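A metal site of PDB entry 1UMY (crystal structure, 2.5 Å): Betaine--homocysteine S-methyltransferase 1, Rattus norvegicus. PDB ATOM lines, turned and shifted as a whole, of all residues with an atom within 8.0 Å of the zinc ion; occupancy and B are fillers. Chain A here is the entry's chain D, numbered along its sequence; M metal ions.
The backbone NH (N) of Ala 250 is in hydrogen-bond range of the backbone carbonyl oxygen (O) of Cys 300 (3.1 Å).
O of Cys 299 sits at hydrogen-bond distance from N of Gly 28, at 3.1 Å.
N of Cys 299 is in hydrogen-bond range of O of Pro 248 (2.7 Å).
The side-chain hydroxyl (OH) of Tyr 160 sits close to the side-chain sulfur (SG) of Cys 217 (3.2 Å).
SG of Cys 217 sits close to ND1 of His 218, 3.3 Å away.
N of Cys 217 is in hydrogen-bond range of O of Gln 247 (3.2 Å).
The side-chain amide oxygen (OD1) of Asn 216 lies within hydrogen-bond range of the backbone NH (N) of Tyr 160, 3.1 Å away.
OH of Tyr 160 touches the zinc ion, 3.2 Å away.
Within 4 Å of the zinc ion: Tyr 160, Cys 217, Cys 299 and Cys 300.
The nearest printed residue that does not touch the zinc ion is Leu 249 (4.4 Å).
The zinc ion is bound by the side-chain sulfur (SG) of Cys 300, the side-chain sulfur (SG) of Cys 299 and the side-chain sulfur (SG) of Cys 217.
Slightly farther from the zinc ion lies N of Cys 300 (2.6 Å).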
ATOM      1  N   GLY A  27       8.640 -30.168  -7.759  1.00  0.00           N
ATOM      2  CA  GLY A  27       9.756 -29.260  -7.951  1.00  0.00           C
ATOM      3  C   GLY A  27       9.534 -27.761  -8.027  1.00  0.00           C
ATOM      4  O   GLY A  27       8.576 -27.228  -7.483  1.00  0.00           O
ATOM      5  N   GLY A  28      10.443 -27.089  -8.726  1.00  0.00           N
ATOM      6  CA  GLY A  28      10.390 -25.642  -8.893  1.00  0.00           C
ATOM      7  C   GLY A  28       9.459 -25.178 -10.003  1.00  0.00           C
ATOM      8  O   GLY A  28       9.914 -24.775 -11.065  1.00  0.00           O
ATOM      9  N   PHE A  29       8.163 -25.236  -9.733  1.00  0.00           N
ATOM     10  CA  PHE A  29       7.167 -24.824 -10.693  1.00  0.00           C
ATOM     11  C   PHE A  29       7.436 -23.457 -11.343  1.00  0.00           C
ATOM     12  O   PHE A  29       7.600 -23.371 -12.561  1.00  0.00           O
ATOM     13  CB  PHE A  29       5.782 -24.797 -10.017  1.00  0.00           C
ATOM     14  CG  PHE A  29       4.683 -25.399 -10.855  1.00  0.00           C
ATOM     15  CD1 PHE A  29       4.560 -26.790 -10.990  1.00  0.00           C
ATOM     16  CD2 PHE A  29       3.765 -24.579 -11.519  1.00  0.00           C
ATOM     17  CE1 PHE A  29       3.555 -27.343 -11.771  1.00  0.00           C
ATOM     18  CE2 PHE A  29       2.750 -25.126 -12.312  1.00  0.00           C
ATOM     19  CZ  PHE A  29       2.646 -26.513 -12.437  1.00  0.00           C
ATOM     20  N   VAL A  30       7.504 -22.404 -10.542  1.00  0.00           N
ATOM     21  CA  VAL A  30       7.727 -21.048 -11.049  1.00  0.00           C
ATOM     22  C   VAL A  30       8.884 -20.859 -12.035  1.00  0.00           C
ATOM     23  O   VAL A  30       8.720 -20.206 -13.072  1.00  0.00           O
ATOM     24  CB  VAL A  30       7.911 -20.069  -9.916  1.00  0.00           C
ATOM     25  CG1 VAL A  30       7.779 -18.652 -10.431  1.00  0.00           C
ATOM     26  CG2 VAL A  30       6.896 -20.363  -8.836  1.00  0.00           C
ATOM     27  N   PHE A  31      10.045 -21.404 -11.711  1.00  0.00           N
ATOM     28  CA  PHE A  31      11.211 -21.300 -12.576  1.00  0.00           C
ATOM     29  C   PHE A  31      11.033 -22.098 -13.860  1.00  0.00           C
ATOM     30  O   PHE A  31      11.457 -21.658 -14.932  1.00  0.00           O
ATOM     31  CB  PHE A  31      12.477 -21.800 -11.844  1.00  0.00           C
ATOM     32  CG  PHE A  31      13.316 -20.693 -11.257  1.00  0.00           C
ATOM     33  CD1 PHE A  31      14.683 -20.857 -11.115  1.00  0.00           C
ATOM     34  CD2 PHE A  31      12.744 -19.494 -10.852  1.00  0.00           C
ATOM     35  CE1 PHE A  31      15.472 -19.829 -10.597  1.00  0.00           C
ATOM     36  CE2 PHE A  31      13.512 -18.475 -10.323  1.00  0.00           C
ATOM     37  CZ  PHE A  31      14.881 -18.641 -10.191  1.00  0.00           C
ATOM     38  N   GLU A 159       6.142 -22.281   3.566  1.00  0.00           N
ATOM     39  CA  GLU A 159       7.465 -22.338   2.954  1.00  0.00           C
ATOM     40  C   GLU A 159       7.906 -20.898   2.916  1.00  0.00           C
ATOM     41  O   GLU A 159       7.181 -20.012   3.379  1.00  0.00           O
ATOM     42  CB  GLU A 159       7.318 -22.868   1.530  1.00  0.00           C
ATOM     43  CG  GLU A 159       6.265 -22.048   0.754  1.00  0.00           C
ATOM     44  CD  GLU A 159       5.926 -22.589  -0.629  1.00  0.00           C
ATOM     45  OE1 GLU A 159       6.847 -22.792  -1.433  1.00  0.00           O
ATOM     46  OE2 GLU A 159       4.730 -22.786  -0.916  1.00  0.00           O
ATOM     47  N   TYR A 160       9.078 -20.660   2.330  1.00  0.00           N
ATOM     48  CA  TYR A 160       9.612 -19.313   2.176  1.00  0.00           C
ATOM     49  C   TYR A 160       9.409 -18.483   3.417  1.00  0.00           C
ATOM     50  O   TYR A 160       8.489 -17.663   3.491  1.00  0.00           O
ATOM     51  CB  TYR A 160       8.930 -18.602   1.008  1.00  0.00           C
ATOM     52  CG  TYR A 160       9.328 -19.046  -0.386  1.00  0.00           C
ATOM     53  CD1 TYR A 160       8.679 -20.112  -1.019  1.00  0.00           C
ATOM     54  CD2 TYR A 160      10.297 -18.346  -1.107  1.00  0.00           C
ATOM     55  CE1 TYR A 160       8.986 -20.461  -2.337  1.00  0.00           C
ATOM     56  CE2 TYR A 160      10.624 -18.693  -2.424  1.00  0.00           C
ATOM     57  CZ  TYR A 160       9.963 -19.745  -3.030  1.00  0.00           C
ATOM     58  OH  TYR A 160      10.308 -20.077  -4.329  1.00  0.00           O
ATOM     59  N   CYS A 186      13.483 -20.593   4.236  1.00  0.00           N
ATOM     60  CA  CYS A 186      14.624 -20.262   3.382  1.00  0.00           C
ATOM     61  C   CYS A 186      15.629 -19.509   4.273  1.00  0.00           C
ATOM     62  O   CYS A 186      15.765 -18.278   4.198  1.00  0.00           O
ATOM     63  CB  CYS A 186      14.191 -19.456   2.129  1.00  0.00           C
ATOM     64  SG  CYS A 186      14.171 -17.580   2.127  1.00  0.00           S
ATOM     65  N   ASN A 216      13.514 -24.951   2.944  1.00  0.00           N
ATOM     66  CA  ASN A 216      13.311 -24.892   1.501  1.00  0.00           C
ATOM     67  C   ASN A 216      13.819 -23.565   0.939  1.00  0.00           C
ATOM     68  O   ASN A 216      13.845 -22.539   1.629  1.00  0.00           O
ATOM     69  CB  ASN A 216      11.820 -24.991   1.172  1.00  0.00           C
ATOM     70  CG  ASN A 216      11.127 -23.638   1.238  1.00  0.00           C
ATOM     71  OD1 ASN A 216      11.106 -22.984   2.294  1.00  0.00           O
ATOM     72  ND2 ASN A 216      10.559 -23.189   0.115  1.00  0.00           N
ATOM     73  N   CYS A 217      14.243 -23.607  -0.315  1.00  0.00           N
ATOM     74  CA  CYS A 217      14.674 -22.387  -0.972  1.00  0.00           C
ATOM     75  C   CYS A 217      15.891 -21.617  -0.470  1.00  0.00           C
ATOM     76  O   CYS A 217      16.047 -21.361   0.737  1.00  0.00           O
ATOM     77  CB  CYS A 217      13.509 -21.410  -1.011  1.00  0.00           C
ATOM     78  SG  CYS A 217      12.915 -21.046  -2.651  1.00  0.00           S
ATOM     79  N   HIS A 218      16.732 -21.223  -1.431  1.00  0.00           N
ATOM     80  CA  HIS A 218      17.920 -20.400  -1.189  1.00  0.00           C
ATOM     81  C   HIS A 218      19.158 -21.047  -0.509  1.00  0.00           C
ATOM     82  O   HIS A 218      19.982 -20.355   0.105  1.00  0.00           O
ATOM     83  CB  HIS A 218      17.467 -19.141  -0.450  1.00  0.00           C
ATOM     84  CG  HIS A 218      16.405 -18.375  -1.184  1.00  0.00           C
ATOM     85  ND1 HIS A 218      15.172 -18.917  -1.491  1.00  0.00           N
ATOM     86  CD2 HIS A 218      16.405 -17.131  -1.723  1.00  0.00           C
ATOM     87  CE1 HIS A 218      14.463 -18.043  -2.194  1.00  0.00           C
ATOM     88  NE2 HIS A 218      15.184 -16.952  -2.341  1.00  0.00           N
ATOM     89  N   PHE A 219      19.272 -22.377  -0.662  1.00  0.00           N
ATOM     90  CA  PHE A 219      20.376 -23.171  -0.103  1.00  0.00           C
ATOM     91  C   PHE A 219      20.435 -24.500  -0.885  1.00  0.00           C
ATOM     92  O   PHE A 219      19.460 -25.292  -0.852  1.00  0.00           O
ATOM     93  CB  PHE A 219      20.138 -23.442   1.407  1.00  0.00           C
ATOM     94  CG  PHE A 219      19.821 -22.183   2.207  1.00  0.00           C
ATOM     95  CD1 PHE A 219      18.501 -21.748   2.348  1.00  0.00           C
ATOM     96  CD2 PHE A 219      20.855 -21.382   2.710  1.00  0.00           C
ATOM     97  CE1 PHE A 219      18.216 -20.516   2.972  1.00  0.00           C
ATOM     98  CE2 PHE A 219      20.591 -20.149   3.335  1.00  0.00           C
ATOM     99  CZ  PHE A 219      19.261 -19.717   3.465  1.00  0.00           C
ATOM    100  N   GLN A 247      13.303 -29.184   0.654  1.00  0.00           N
ATOM    101  CA  GLN A 247      13.031 -28.885  -0.754  1.00  0.00           C
ATOM    102  C   GLN A 247      13.993 -27.783  -1.091  1.00  0.00           C
ATOM    103  O   GLN A 247      13.640 -26.613  -1.146  1.00  0.00           O
ATOM    104  CB  GLN A 247      11.596 -28.414  -0.927  1.00  0.00           C
ATOM    105  CG  GLN A 247      10.565 -29.443  -0.518  1.00  0.00           C
ATOM    106  CD  GLN A 247       9.181 -29.135  -1.072  1.00  0.00           C
ATOM    107  OE1 GLN A 247       8.649 -28.027  -0.900  1.00  0.00           O
ATOM    108  NE2 GLN A 247       8.580 -30.117  -1.751  1.00  0.00           N
ATOM    109  N   PRO A 248      15.263 -28.136  -1.315  1.00  0.00           N
ATOM    110  CA  PRO A 248      16.347 -27.222  -1.654  1.00  0.00           C
ATOM    111  C   PRO A 248      16.428 -26.758  -3.094  1.00  0.00           C
ATOM    112  O   PRO A 248      15.628 -27.143  -3.948  1.00  0.00           O
ATOM    113  CB  PRO A 248      17.582 -28.021  -1.290  1.00  0.00           C
ATOM    114  CG  PRO A 248      17.185 -29.404  -1.744  1.00  0.00           C
ATOM    115  CD  PRO A 248      15.757 -29.521  -1.203  1.00  0.00           C
ATOM    116  N   LEU A 249      17.432 -25.912  -3.352  1.00  0.00           N
ATOM    117  CA  LEU A 249      17.686 -25.416  -4.684  1.00  0.00           C
ATOM    118  C   LEU A 249      18.335 -26.559  -5.456  1.00  0.00           C
ATOM    119  O   LEU A 249      18.901 -27.462  -4.849  1.00  0.00           O
ATOM    120  CB  LEU A 249      18.673 -24.256  -4.633  1.00  0.00           C
ATOM    121  CG  LEU A 249      18.365 -23.034  -3.773  1.00  0.00           C
ATOM    122  CD1 LEU A 249      19.571 -22.079  -3.815  1.00  0.00           C
ATOM    123  CD2 LEU A 249      17.136 -22.350  -4.286  1.00  0.00           C
ATOM    124  N   ALA A 250      18.246 -26.518  -6.774  1.00  0.00           N
ATOM    125  CA  ALA A 250      18.880 -27.549  -7.592  1.00  0.00           C
ATOM    126  C   ALA A 250      20.150 -26.879  -8.101  1.00  0.00           C
ATOM    127  O   ALA A 250      20.806 -27.361  -9.037  1.00  0.00           O
ATOM    128  CB  ALA A 250      17.987 -27.945  -8.748  1.00  0.00           C
ATOM    129  N   TYR A 251      20.495 -25.766  -7.468  1.00  0.00           N
ATOM    130  CA  TYR A 251      21.669 -24.985  -7.824  1.00  0.00           C
ATOM    131  C   TYR A 251      22.784 -25.120  -6.802  1.00  0.00           C
ATOM    132  O   TYR A 251      22.557 -24.960  -5.612  1.00  0.00           O
ATOM    133  CB  TYR A 251      21.280 -23.514  -7.947  1.00  0.00           C
ATOM    134  CG  TYR A 251      20.281 -23.255  -9.038  1.00  0.00           C
ATOM    135  CD1 TYR A 251      20.637 -23.410 -10.375  1.00  0.00           C
ATOM    136  CD2 TYR A 251      18.975 -22.876  -8.741  1.00  0.00           C
ATOM    137  CE1 TYR A 251      19.707 -23.192 -11.391  1.00  0.00           C
ATOM    138  CE2 TYR A 251      18.044 -22.656  -9.747  1.00  0.00           C
ATOM    139  CZ  TYR A 251      18.410 -22.819 -11.071  1.00  0.00           C
ATOM    140  OH  TYR A 251      17.499 -22.607 -12.074  1.00  0.00           O
ATOM    141  N   PHE A 261      20.627 -17.613  -2.706  1.00  0.00           N
ATOM    142  CA  PHE A 261      21.265 -17.362  -3.989  1.00  0.00           C
ATOM    143  C   PHE A 261      20.771 -16.105  -4.678  1.00  0.00           C
ATOM    144  O   PHE A 261      21.269 -15.749  -5.727  1.00  0.00           O
ATOM    145  CB  PHE A 261      21.124 -18.565  -4.936  1.00  0.00           C
ATOM    146  CG  PHE A 261      19.733 -18.809  -5.432  1.00  0.00           C
ATOM    147  CD1 PHE A 261      19.542 -19.460  -6.657  1.00  0.00           C
ATOM    148  CD2 PHE A 261      18.623 -18.444  -4.687  1.00  0.00           C
ATOM    149  CE1 PHE A 261      18.261 -19.724  -7.131  1.00  0.00           C
ATOM    150  CE2 PHE A 261      17.332 -18.707  -5.151  1.00  0.00           C
ATOM    151  CZ  PHE A 261      17.151 -19.348  -6.378  1.00  0.00           C
ATOM    152  N   PHE A 267      21.909 -14.454 -10.202  1.00  0.00           N
ATOM    153  CA  PHE A 267      20.470 -14.558 -10.014  1.00  0.00           C
ATOM    154  C   PHE A 267      19.743 -13.491 -10.811  1.00  0.00           C
ATOM    155  O   PHE A 267      20.041 -12.308 -10.680  1.00  0.00           O
ATOM    156  CB  PHE A 267      20.086 -14.413  -8.534  1.00  0.00           C
ATOM    157  CG  PHE A 267      18.606 -14.558  -8.288  1.00  0.00           C
ATOM    158  CD1 PHE A 267      18.020 -15.812  -8.209  1.00  0.00           C
ATOM    159  CD2 PHE A 267      17.788 -13.437  -8.221  1.00  0.00           C
ATOM    160  CE1 PHE A 267      16.646 -15.947  -8.081  1.00  0.00           C
ATOM    161  CE2 PHE A 267      16.415 -13.574  -8.103  1.00  0.00           C
ATOM    162  CZ  PHE A 267      15.849 -14.829  -8.032  1.00  0.00           C
ATOM    163  N   GLY A 298      11.962 -30.558  -3.921  1.00  0.00           N
ATOM    164  CA  GLY A 298      12.922 -29.594  -4.423  1.00  0.00           C
ATOM    165  C   GLY A 298      12.277 -28.247  -4.671  1.00  0.00           C
ATOM    166  O   GLY A 298      11.066 -28.159  -4.826  1.00  0.00           O
ATOM    167  N   CYS A 299      13.085 -27.198  -4.710  1.00  0.00           N
ATOM    168  CA  CYS A 299      12.581 -25.861  -4.946  1.00  0.00           C
ATOM    169  C   CYS A 299      13.016 -25.344  -6.321  1.00  0.00           C
ATOM    170  O   CYS A 299      13.039 -26.103  -7.292  1.00  0.00           O
ATOM    171  CB  CYS A 299      13.093 -24.947  -3.858  1.00  0.00           C
ATOM    172  SG  CYS A 299      11.926 -23.672  -3.480  1.00  0.00           S
ATOM    173  N   CYS A 300      13.371 -24.072  -6.400  1.00  0.00           N
ATOM    174  CA  CYS A 300      13.806 -23.490  -7.666  1.00  0.00           C
ATOM    175  C   CYS A 300      14.901 -24.331  -8.339  1.00  0.00           C
ATOM    176  O   CYS A 300      15.847 -24.782  -7.681  1.00  0.00           O
ATOM    177  CB  CYS A 300      14.335 -22.072  -7.457  1.00  0.00           C
ATOM    178  SG  CYS A 300      13.072 -20.831  -7.119  1.00  0.00           S
ATOM    179  N   GLY A 301      14.777 -24.536  -9.647  1.00  0.00           N
ATOM    180  CA  GLY A 301      15.752 -25.316 -10.383  1.00  0.00           C
ATOM    181  C   GLY A 301      15.366 -26.778 -10.593  1.00  0.00           C
ATOM    182  O   GLY A 301      15.830 -27.414 -11.529  1.00  0.00           O
ATOM    183  N   PHE A 302      14.519 -27.318  -9.734  1.00  0.00           N
ATOM    184  CA  PHE A 302      14.116 -28.701  -9.911  1.00  0.00           C
ATOM    185  C   PHE A 302      13.203 -28.885 -11.125  1.00  0.00           C
ATOM    186  O   PHE A 302      12.106 -28.338 -11.178  1.00  0.00           O
ATOM    187  CB  PHE A 302      13.379 -29.227  -8.689  1.00  0.00           C
ATOM    188  CG  PHE A 302      14.263 -29.825  -7.664  1.00  0.00           C
ATOM    189  CD1 PHE A 302      15.124 -29.039  -6.914  1.00  0.00           C
ATOM    190  CD2 PHE A 302      14.258 -31.193  -7.448  1.00  0.00           C
ATOM    191  CE1 PHE A 302      15.959 -29.595  -5.964  1.00  0.00           C
ATOM    192  CE2 PHE A 302      15.086 -31.763  -6.516  1.00  0.00           C
ATOM    193  CZ  PHE A 302      15.946 -30.968  -5.767  1.00  0.00           C
HETATM  194 ZN    ZN M   1      12.813 -21.950  -4.985  1.00  0.00          ZN
